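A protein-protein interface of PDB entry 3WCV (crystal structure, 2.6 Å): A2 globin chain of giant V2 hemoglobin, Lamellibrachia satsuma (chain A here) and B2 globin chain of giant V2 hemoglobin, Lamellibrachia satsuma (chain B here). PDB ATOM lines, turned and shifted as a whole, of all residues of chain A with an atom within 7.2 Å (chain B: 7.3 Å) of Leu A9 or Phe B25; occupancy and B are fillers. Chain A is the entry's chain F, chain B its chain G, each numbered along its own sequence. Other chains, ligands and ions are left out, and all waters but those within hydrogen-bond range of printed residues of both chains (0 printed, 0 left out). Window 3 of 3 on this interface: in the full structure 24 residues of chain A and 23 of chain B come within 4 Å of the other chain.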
ATOM      1  N   CYS A   3      13.251  21.221 -23.276  1.00  0.00           N
ATOM      2  CA  CYS A   3      14.415  20.360 -23.392  1.00  0.00           C
ATOM      3  C   CYS A   3      15.585  21.206 -23.901  1.00  0.00           C
ATOM      4  O   CYS A   3      16.049  21.043 -25.038  1.00  0.00           O
ATOM      5  CB  CYS A   3      14.151  19.188 -24.347  1.00  0.00           C
ATOM      6  SG  CYS A   3      15.586  18.077 -24.514  1.00  0.00           S
ATOM      7  N   GLY A   4      16.040  22.120 -23.039  1.00  0.00           N
ATOM      8  CA  GLY A   4      17.150  22.993 -23.355  1.00  0.00           C
ATOM      9  C   GLY A   4      18.444  22.210 -23.324  1.00  0.00           C
ATOM     10  O   GLY A   4      18.422  20.996 -23.130  1.00  0.00           O
ATOM     11  N   PRO A   5      19.590  22.875 -23.512  1.00  0.00           N
ATOM     12  CA  PRO A   5      20.906  22.219 -23.509  1.00  0.00           C
ATOM     13  C   PRO A   5      21.242  21.478 -22.218  1.00  0.00           C
ATOM     14  O   PRO A   5      21.808  20.379 -22.247  1.00  0.00           O
ATOM     15  CB  PRO A   5      21.872  23.372 -23.775  1.00  0.00           C
ATOM     16  CG  PRO A   5      21.029  24.312 -24.606  1.00  0.00           C
ATOM     17  CD  PRO A   5      19.718  24.297 -23.862  1.00  0.00           C
ATOM     18  N   LEU A   6      20.883  22.083 -21.085  1.00  0.00           N
ATOM     19  CA  LEU A   6      21.173  21.495 -19.786  1.00  0.00           C
ATOM     20  C   LEU A   6      20.397  20.197 -19.581  1.00  0.00           C
ATOM     21  O   LEU A   6      20.985  19.170 -19.243  1.00  0.00           O
ATOM     22  CB  LEU A   6      20.882  22.520 -18.676  1.00  0.00           C
ATOM     23  CG  LEU A   6      21.650  23.856 -18.810  1.00  0.00           C
ATOM     24  CD1 LEU A   6      21.288  24.799 -17.669  1.00  0.00           C
ATOM     25  CD2 LEU A   6      23.162  23.604 -18.814  1.00  0.00           C
ATOM     26  N   GLN A   7      19.089  20.229 -19.812  1.00  0.00           N
ATOM     27  CA  GLN A   7      18.256  19.036 -19.657  1.00  0.00           C
ATOM     28  C   GLN A   7      18.762  17.905 -20.540  1.00  0.00           C
ATOM     29  O   GLN A   7      18.626  16.733 -20.195  1.00  0.00           O
ATOM     30  CB  GLN A   7      16.803  19.326 -20.026  1.00  0.00           C
ATOM     31  CG  GLN A   7      16.086  20.315 -19.126  1.00  0.00           C
ATOM     32  CD  GLN A   7      16.640  21.734 -19.231  1.00  0.00           C
ATOM     33  OE1 GLN A   7      17.064  22.185 -20.303  1.00  0.00           O
ATOM     34  NE2 GLN A   7      16.612  22.450 -18.120  1.00  0.00           N
ATOM     35  N   ARG A   8      19.347  18.259 -21.676  1.00  0.00           N
ATOM     36  CA  ARG A   8      19.847  17.261 -22.602  1.00  0.00           C
ATOM     37  C   ARG A   8      21.126  16.615 -22.094  1.00  0.00           C
ATOM     38  O   ARG A   8      21.388  15.440 -22.358  1.00  0.00           O
ATOM     39  CB  ARG A   8      20.071  17.889 -23.988  1.00  0.00           C
ATOM     40  CG  ARG A   8      18.768  18.325 -24.664  1.00  0.00           C
ATOM     41  CD  ARG A   8      19.005  19.129 -25.933  1.00  0.00           C
ATOM     42  NE  ARG A   8      17.760  19.682 -26.473  1.00  0.00           N
ATOM     43  CZ  ARG A   8      17.177  19.276 -27.599  1.00  0.00           C
ATOM     44  NH1 ARG A   8      17.718  18.309 -28.336  1.00  0.00           N
ATOM     45  NH2 ARG A   8      16.037  19.826 -27.988  1.00  0.00           N
ATOM     46  N   LEU A   9      21.936  17.373 -21.368  1.00  0.00           N
ATOM     47  CA  LEU A   9      23.151  16.792 -20.841  1.00  0.00           C
ATOM     48  C   LEU A   9      22.719  15.890 -19.697  1.00  0.00           C
ATOM     49  O   LEU A   9      23.181  14.759 -19.589  1.00  0.00           O
ATOM     50  CB  LEU A   9      24.084  17.874 -20.314  1.00  0.00           C
ATOM     51  CG  LEU A   9      24.863  18.698 -21.333  1.00  0.00           C
ATOM     52  CD1 LEU A   9      25.695  19.758 -20.601  1.00  0.00           C
ATOM     53  CD2 LEU A   9      25.759  17.797 -22.162  1.00  0.00           C
ATOM     54  N   LYS A  10      21.821  16.419 -18.863  1.00  0.00           N
ATOM     55  CA  LYS A  10      21.299  15.720 -17.703  1.00  0.00           C
ATOM     56  C   LYS A  10      20.739  14.386 -18.144  1.00  0.00           C
ATOM     57  O   LYS A  10      21.143  13.343 -17.639  1.00  0.00           O
ATOM     58  CB  LYS A  10      20.183  16.533 -17.040  1.00  0.00           C
ATOM     59  CG  LYS A  10      19.704  16.005 -15.688  1.00  0.00           C
ATOM     60  CD  LYS A  10      20.669  16.444 -14.589  1.00  0.00           C
ATOM     61  CE  LYS A  10      20.156  16.109 -13.198  1.00  0.00           C
ATOM     62  NZ  LYS A  10      19.132  17.064 -12.744  1.00  0.00           N
ATOM     63  N   VAL A  11      19.814  14.437 -19.105  1.00  0.00           N
ATOM     64  CA  VAL A  11      19.170  13.245 -19.647  1.00  0.00           C
ATOM     65  C   VAL A  11      20.207  12.270 -20.211  1.00  0.00           C
ATOM     66  O   VAL A  11      20.096  11.053 -20.023  1.00  0.00           O
ATOM     67  CB  VAL A  11      18.101  13.650 -20.742  1.00  0.00           C
ATOM     68  CG1 VAL A  11      17.626  12.451 -21.548  1.00  0.00           C
ATOM     69  CG2 VAL A  11      16.908  14.263 -20.058  1.00  0.00           C
ATOM     70  N   LYS A  12      21.212  12.803 -20.896  1.00  0.00           N
ATOM     71  CA  LYS A  12      22.282  11.969 -21.459  1.00  0.00           C
ATOM     72  C   LYS A  12      23.013  11.213 -20.359  1.00  0.00           C
ATOM     73  O   LYS A  12      23.366  10.043 -20.514  1.00  0.00           O
ATOM     74  CB  LYS A  12      23.306  12.820 -22.199  1.00  0.00           C
ATOM     75  CG  LYS A  12      22.970  13.130 -23.628  1.00  0.00           C
ATOM     76  CD  LYS A  12      23.925  14.207 -24.109  1.00  0.00           C
ATOM     77  CE  LYS A  12      23.710  14.548 -25.563  1.00  0.00           C
ATOM     78  NZ  LYS A  12      23.969  13.370 -26.436  1.00  0.00           N
ATOM     79  N   ARG A  13      23.239  11.895 -19.248  1.00  0.00           N
ATOM     80  CA  ARG A  13      23.931  11.277 -18.142  1.00  0.00           C
ATOM     81  C   ARG A  13      23.066  10.229 -17.453  1.00  0.00           C
ATOM     82  O   ARG A  13      23.485   9.086 -17.330  1.00  0.00           O
ATOM     83  CB  ARG A  13      24.404  12.332 -17.131  1.00  0.00           C
ATOM     84  CG  ARG A  13      25.389  11.777 -16.114  1.00  0.00           C
ATOM     85  CD  ARG A  13      26.146  12.884 -15.403  1.00  0.00           C
ATOM     86  NE  ARG A  13      25.203  13.811 -14.804  1.00  0.00           N
ATOM     87  CZ  ARG A  13      24.381  13.492 -13.811  1.00  0.00           C
ATOM     88  NH1 ARG A  13      23.541  14.403 -13.331  1.00  0.00           N
ATOM     89  NH2 ARG A  13      24.422  12.273 -13.289  1.00  0.00           N
ATOM     90  N   GLN A  14      21.865  10.604 -17.024  1.00  0.00           N
ATOM     91  CA  GLN A  14      21.004   9.665 -16.333  1.00  0.00           C
ATOM     92  C   GLN A  14      20.657   8.488 -17.205  1.00  0.00           C
ATOM     93  O   GLN A  14      20.440   7.387 -16.706  1.00  0.00           O
ATOM     94  CB  GLN A  14      19.748  10.358 -15.835  1.00  0.00           C
ATOM     95  CG  GLN A  14      20.074  11.528 -14.938  1.00  0.00           C
ATOM     96  CD  GLN A  14      18.889  11.970 -14.079  1.00  0.00           C
ATOM     97  OE1 GLN A  14      17.746  11.977 -14.534  1.00  0.00           O
ATOM     98  NE2 GLN A  14      19.168  12.352 -12.834  1.00  0.00           N
ATOM     99  N   TRP A  15      20.637   8.704 -18.511  1.00  0.00           N
ATOM    100  CA  TRP A  15      20.349   7.603 -19.409  1.00  0.00           C
ATOM    101  C   TRP A  15      21.563   6.671 -19.468  1.00  0.00           C
ATOM    102  O   TRP A  15      21.399   5.462 -19.432  1.00  0.00           O
ATOM    103  CB  TRP A  15      19.984   8.112 -20.818  1.00  0.00           C
ATOM    104  CG  TRP A  15      20.005   7.034 -21.862  1.00  0.00           C
ATOM    105  CD1 TRP A  15      21.010   6.782 -22.752  1.00  0.00           C
ATOM    106  CD2 TRP A  15      19.013   6.019 -22.078  1.00  0.00           C
ATOM    107  NE1 TRP A  15      20.709   5.674 -23.507  1.00  0.00           N
ATOM    108  CE2 TRP A  15      19.489   5.188 -23.116  1.00  0.00           C
ATOM    109  CE3 TRP A  15      17.773   5.733 -21.498  1.00  0.00           C
ATOM    110  CZ2 TRP A  15      18.770   4.091 -23.585  1.00  0.00           C
ATOM    111  CZ3 TRP A  15      17.057   4.638 -21.966  1.00  0.00           C
ATOM    112  CH2 TRP A  15      17.561   3.833 -22.999  1.00  0.00           C
ATOM    113  N   ALA A  16      22.768   7.226 -19.528  1.00  0.00           N
ATOM    114  CA  ALA A  16      23.978   6.394 -19.591  1.00  0.00           C
ATOM    115  C   ALA A  16      24.140   5.527 -18.346  1.00  0.00           C
ATOM    116  O   ALA A  16      24.750   4.448 -18.387  1.00  0.00           O
ATOM    117  CB  ALA A  16      25.192   7.252 -19.771  1.00  0.00           C
ATOM    118  N   ASP A  72      18.462   5.101 -27.224  1.00  0.00           N
ATOM    119  CA  ASP A  72      19.850   5.442 -27.037  1.00  0.00           C
ATOM    120  C   ASP A  72      20.351   6.364 -28.135  1.00  0.00           C
ATOM    121  O   ASP A  72      20.981   7.388 -27.844  1.00  0.00           O
ATOM    122  CB  ASP A  72      20.693   4.180 -26.989  1.00  0.00           C
ATOM    123  CG  ASP A  72      22.134   4.466 -26.663  1.00  0.00           C
ATOM    124  OD1 ASP A  72      22.971   4.427 -27.588  1.00  0.00           O
ATOM    125  OD2 ASP A  72      22.421   4.746 -25.479  1.00  0.00           O
ATOM    126  N   VAL A  75      18.981   9.886 -27.634  1.00  0.00           N
ATOM    127  CA  VAL A  75      19.602  10.485 -26.468  1.00  0.00           C
ATOM    128  C   VAL A  75      21.036  10.886 -26.818  1.00  0.00           C
ATOM    129  O   VAL A  75      21.477  12.002 -26.536  1.00  0.00           O
ATOM    130  CB  VAL A  75      19.589   9.478 -25.301  1.00  0.00           C
ATOM    131  CG1 VAL A  75      20.590   9.886 -24.222  1.00  0.00           C
ATOM    132  CG2 VAL A  75      18.182   9.403 -24.719  1.00  0.00           C
ATOM    133  N   ALA A  76      21.746   9.964 -27.457  1.00  0.00           N
ATOM    134  CA  ALA A  76      23.122  10.204 -27.838  1.00  0.00           C
ATOM    135  C   ALA A  76      23.212  11.409 -28.779  1.00  0.00           C
ATOM    136  O   ALA A  76      24.231  12.113 -28.811  1.00  0.00           O
ATOM    137  CB  ALA A  76      23.692   8.958 -28.511  1.00  0.00           C
ATOM    138  N   LEU A  77      22.133  11.647 -29.531  1.00  0.00           N
ATOM    139  CA  LEU A  77      22.092  12.748 -30.481  1.00  0.00           C
ATOM    140  C   LEU A  77      21.364  14.018 -30.040  1.00  0.00           C
ATOM    141  O   LEU A  77      21.254  14.956 -30.823  1.00  0.00           O
ATOM    142  CB  LEU A  77      21.501  12.263 -31.797  1.00  0.00           C
ATOM    143  CG  LEU A  77      22.342  11.213 -32.515  1.00  0.00           C
ATOM    144  CD1 LEU A  77      21.542  10.601 -33.668  1.00  0.00           C
ATOM    145  CD2 LEU A  77      23.624  11.861 -33.005  1.00  0.00           C
ATOM    146  N   LEU A  78      20.869  14.069 -28.808  1.00  0.00           N
ATOM    147  CA  LEU A  78      20.179  15.271 -28.342  1.00  0.00           C
ATOM    148  C   LEU A  78      21.011  16.553 -28.513  1.00  0.00           C
ATOM    149  O   LEU A  78      20.482  17.662 -28.465  1.00  0.00           O
ATOM    150  CB  LEU A  78      19.794  15.116 -26.871  1.00  0.00           C
ATOM    151  CG  LEU A  78      18.740  14.050 -26.615  1.00  0.00           C
ATOM    152  CD1 LEU A  78      18.572  13.862 -25.124  1.00  0.00           C
ATOM    153  CD2 LEU A  78      17.413  14.466 -27.283  1.00  0.00           C
ATOM    154  N   ASP A  79      22.309  16.404 -28.722  1.00  0.00           N
ATOM    155  CA  ASP A  79      23.181  17.563 -28.847  1.00  0.00           C
ATOM    156  C   ASP A  79      23.520  17.902 -30.293  1.00  0.00           C
ATOM    157  O   ASP A  79      24.226  18.878 -30.556  1.00  0.00           O
ATOM    158  CB  ASP A  79      24.469  17.327 -28.034  1.00  0.00           C
ATOM    159  CG  ASP A  79      25.274  16.145 -28.541  1.00  0.00           C
ATOM    160  OD1 ASP A  79      26.355  16.367 -29.126  1.00  0.00           O
ATOM    161  OD2 ASP A  79      24.833  14.988 -28.369  1.00  0.00           O
ATOM    162  N   CYS A 133      12.497  16.295 -22.710  1.00  0.00           N
ATOM    163  CA  CYS A 133      13.235  15.702 -23.809  1.00  0.00           C
ATOM    164  C   CYS A 133      12.618  14.474 -24.462  1.00  0.00           C
ATOM    165  O   CYS A 133      12.900  14.196 -25.630  1.00  0.00           O
ATOM    166  CB  CYS A 133      14.663  15.405 -23.369  1.00  0.00           C
ATOM    167  SG  CYS A 133      15.552  16.891 -22.849  1.00  0.00           S
ATOM    168  N   TRP B  21      33.332   2.877 -26.781  1.00  0.00           N
ATOM    169  CA  TRP B  21      31.901   3.020 -27.005  1.00  0.00           C
ATOM    170  C   TRP B  21      31.308   3.962 -25.968  1.00  0.00           C
ATOM    171  O   TRP B  21      30.800   3.515 -24.948  1.00  0.00           O
ATOM    172  CB  TRP B  21      31.229   1.658 -26.898  1.00  0.00           C
ATOM    173  CG  TRP B  21      29.767   1.674 -27.243  1.00  0.00           C
ATOM    174  CD1 TRP B  21      29.201   1.500 -28.481  1.00  0.00           C
ATOM    175  CD2 TRP B  21      28.685   1.907 -26.341  1.00  0.00           C
ATOM    176  NE1 TRP B  21      27.825   1.615 -28.401  1.00  0.00           N
ATOM    177  CE2 TRP B  21      27.483   1.865 -27.097  1.00  0.00           C
ATOM    178  CE3 TRP B  21      28.610   2.150 -24.967  1.00  0.00           C
ATOM    179  CZ2 TRP B  21      26.222   2.058 -26.516  1.00  0.00           C
ATOM    180  CZ3 TRP B  21      27.351   2.345 -24.388  1.00  0.00           C
ATOM    181  CH2 TRP B  21      26.177   2.298 -25.165  1.00  0.00           C
ATOM    182  N   SER B  22      31.375   5.266 -26.242  1.00  0.00           N
ATOM    183  CA  SER B  22      30.847   6.274 -25.317  1.00  0.00           C
ATOM    184  C   SER B  22      29.332   6.139 -25.196  1.00  0.00           C
ATOM    185  O   SER B  22      28.614   6.226 -26.195  1.00  0.00           O
ATOM    186  CB  SER B  22      31.190   7.696 -25.791  1.00  0.00           C
ATOM    187  OG  SER B  22      30.645   7.942 -27.070  1.00  0.00           O
ATOM    188  N   ALA B  23      28.849   5.935 -23.974  1.00  0.00           N
ATOM    189  CA  ALA B  23      27.416   5.769 -23.726  1.00  0.00           C
ATOM    190  C   ALA B  23      26.596   7.069 -23.656  1.00  0.00           C
ATOM    191  O   ALA B  23      25.367   7.020 -23.537  1.00  0.00           O
ATOM    192  CB  ALA B  23      27.215   4.967 -22.444  1.00  0.00           C
ATOM    193  N   GLN B  24      27.268   8.218 -23.752  1.00  0.00           N
ATOM    194  CA  GLN B  24      26.595   9.514 -23.660  1.00  0.00           C
ATOM    195  C   GLN B  24      26.556  10.370 -24.921  1.00  0.00           C
ATOM    196  O   GLN B  24      25.596  11.115 -25.138  1.00  0.00           O
ATOM    197  CB  GLN B  24      27.212  10.342 -22.530  1.00  0.00           C
ATOM    198  CG  GLN B  24      26.668  10.008 -21.152  1.00  0.00           C
ATOM    199  CD  GLN B  24      27.135  10.983 -20.089  1.00  0.00           C
ATOM    200  OE1 GLN B  24      27.069  12.200 -20.273  1.00  0.00           O
ATOM    201  NE2 GLN B  24      27.606  10.454 -18.962  1.00  0.00           N
ATOM    202  N   PHE B  25      27.605  10.284 -25.733  1.00  0.00           N
ATOM    203  CA  PHE B  25      27.685  11.057 -26.967  1.00  0.00           C
ATOM    204  C   PHE B  25      27.994  10.147 -28.129  1.00  0.00           C
ATOM    205  O   PHE B  25      28.309   8.974 -27.943  1.00  0.00           O
ATOM    206  CB  PHE B  25      28.755  12.145 -26.856  1.00  0.00           C
ATOM    207  CG  PHE B  25      28.388  13.244 -25.911  1.00  0.00           C
ATOM    208  CD1 PHE B  25      27.654  14.344 -26.346  1.00  0.00           C
ATOM    209  CD2 PHE B  25      28.725  13.152 -24.565  1.00  0.00           C
ATOM    210  CE1 PHE B  25      27.256  15.337 -25.450  1.00  0.00           C
ATOM    211  CE2 PHE B  25      28.334  14.136 -23.660  1.00  0.00           C
ATOM    212  CZ  PHE B  25      27.596  15.231 -24.102  1.00  0.00           C
ATOM    213  N   THR B  26      27.914  10.702 -29.328  1.00  0.00           N
ATOM    214  CA  THR B  26      28.142   9.941 -30.545  1.00  0.00           C
ATOM    215  C   THR B  26      29.460  10.232 -31.241  1.00  0.00           C
ATOM    216  O   THR B  26      29.835   9.539 -32.187  1.00  0.00           O
ATOM    217  CB  THR B  26      26.999  10.201 -31.539  1.00  0.00           C
ATOM    218  OG1 THR B  26      26.809  11.616 -31.690  1.00  0.00           O
ATOM    219  CG2 THR B  26      25.710   9.577 -31.034  1.00  0.00           C
ATOM    220  N   GLY B  27      30.168  11.250 -30.771  1.00  0.00           N
ATOM    221  CA  GLY B  27      31.429  11.612 -31.398  1.00  0.00           C
ATOM    222  C   GLY B  27      32.318  10.423 -31.664  1.00  0.00           C
ATOM    223  O   GLY B  27      32.779  10.218 -32.787  1.00  0.00           O
ATOM    224  N   ARG B  28      32.545   9.638 -30.619  1.00  0.00           N
ATOM    225  CA  ARG B  28      33.400   8.462 -30.692  1.00  0.00           C
ATOM    226  C   ARG B  28      32.792   7.383 -31.583  1.00  0.00           C
ATOM    227  O   ARG B  28      33.485   6.765 -32.400  1.00  0.00           O
ATOM    228  CB  ARG B  28      33.621   7.936 -29.273  1.00  0.00           C
ATOM    229  CG  ARG B  28      34.940   7.214 -29.056  1.00  0.00           C
ATOM    230  CD  ARG B  28      35.501   7.539 -27.676  1.00  0.00           C
ATOM    231  NE  ARG B  28      34.633   7.083 -26.591  1.00  0.00           N
ATOM    232  CZ  ARG B  28      34.423   7.757 -25.458  1.00  0.00           C
ATOM    233  NH1 ARG B  28      33.625   7.263 -24.518  1.00  0.00           N
ATOM    234  NH2 ARG B  28      34.998   8.940 -25.269  1.00  0.00           N
ATOM    235  N   ARG B  29      31.489   7.165 -31.428  1.00  0.00           N
ATOM    236  CA  ARG B  29      30.790   6.153 -32.220  1.00  0.00           C
ATOM    237  C   ARG B  29      30.919   6.448 -33.712  1.00  0.00           C
ATOM    238  O   ARG B  29      31.243   5.574 -34.523  1.00  0.00           O
ATOM    239  CB  ARG B  29      29.303   6.129 -31.855  1.00  0.00           C
ATOM    240  CG  ARG B  29      29.010   5.982 -30.399  1.00  0.00           C
ATOM    241  CD  ARG B  29      27.521   5.875 -30.178  1.00  0.00           C
ATOM    242  NE  ARG B  29      27.179   5.865 -28.764  1.00  0.00           N
ATOM    243  CZ  ARG B  29      25.941   5.732 -28.307  1.00  0.00           C
ATOM    244  NH1 ARG B  29      24.936   5.593 -29.162  1.00  0.00           N
ATOM    245  NH2 ARG B  29      25.708   5.729 -27.000  1.00  0.00           N
ATOM    246  N   LEU B  30      30.668   7.707 -34.049  1.00  0.00           N
ATOM    247  CA  LEU B  30      30.690   8.174 -35.422  1.00  0.00           C
ATOM    248  C   LEU B  30      32.046   8.017 -36.057  1.00  0.00           C
ATOM    249  O   LEU B  30      32.174   7.461 -37.135  1.00  0.00           O
ATOM    250  CB  LEU B  30      30.254   9.640 -35.447  1.00  0.00           C
ATOM    251  CG  LEU B  30      29.477  10.183 -36.642  1.00  0.00           C
ATOM    252  CD1 LEU B  30      28.326   9.255 -36.973  1.00  0.00           C
ATOM    253  CD2 LEU B  30      28.956  11.565 -36.311  1.00  0.00           C
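O of Gln B24 lies within hydrogen-bond range of NZ of Lys A12 (3.1 Å). The guanidinium group (NH1) of Arg B29 lies within salt-bridge range of the side-chain carboxylate (OD1) of Asp A72, at 2.8 Å.
The backbone carbonyl oxygen (O) of Val A75 lies within hydrogen-bond range of the side-chain amino group (NZ) of Lys A12 (2.8 Å). NZ of Lys A12 lies within hydrogen-bond range of O of Ala A76 (2.7 Å). The side-chain amino group (NZ) of Lys A12 is in salt-bridge range of the side-chain carboxylate (OD2) of Asp A79, 2.7 Å away. NE1 of Trp A15 is in hydrogen-bond range of OD2 of Asp A72, 2.8 Å away. The backbone carbonyl oxygen of Phe B25 sits at hydrogen-bond distance from the side-chain hydroxyl of Ser B22 (2.7 Å). NE of Arg B29 sits at hydrogen-bond distance from O of Ser B22 (3.0 Å).
Among the printed residues, merely in contact across the chains: Leu A9 with Phe B25 (3.7 Å), Lys A12 with Phe B25 (3.6 Å), Arg A13 with Gln B24 (3.8 Å), Ala A16 with Ala B23 (3.8 Å), Ala A16 with Gln B24 (3.4 Å), Ala A76 with Gln B24 (3.8 Å), Ala A76 with Thr B26 (3.3 Å), Ala A76 with Arg B29 (3.6 Å), Leu A77 with Thr B26 (3.5 Å) and Asp A79 with Phe B25 (3.5 Å).
Leu A9 touches just one residue of chain B: Phe B25. Of chain A, only Leu A9, Lys A12 and Asp A79 come within 4 Å of Phe B25. Of the printed residues of chain B, Asp A72 touches Arg B29 (2.8 Å). Printed residues of chain B within 4 Å of Arg A13: Gln B24 (3.8 Å). Of the printed residues of chain B, Asp A79 touches Phe B25. Of the printed residues of chain B, Leu A77 touches Thr B26 (3.5 Å). Of the printed residues of chain B, Ala A16 touches Ala B23 (3.8 Å) and Gln B24 (3.4 Å). Val A75 touches none of the printed residues of chain B. Ser B22 touches none of the printed residues of chain A. The nearest residue of chain B that does not touch Leu A9 is Gln B24 (4.7 Å). The nearest printed residue of chain B that does not touch Leu A77 is Gln B24 (5.6 Å).
Of the 10 printed residues of chain B, 5 touch a printed residue of chain A. Printed residues of chain B that touch a printed residue of chain A: Ala B23, Gln B24, Phe B25, Thr B26 and Arg B29. Hydrophobic or aromatic side chains of chain B within 4 Å of the printed part of chain A: Phe B25. Among the printed residues, 12 pairs touch across the chains. Among the printed residues, Asp or Glu carboxylates within 4 Å of a Lys or Arg side-chain nitrogen of the other chain: Asp A72 with Arg B29 (2.8 Å).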
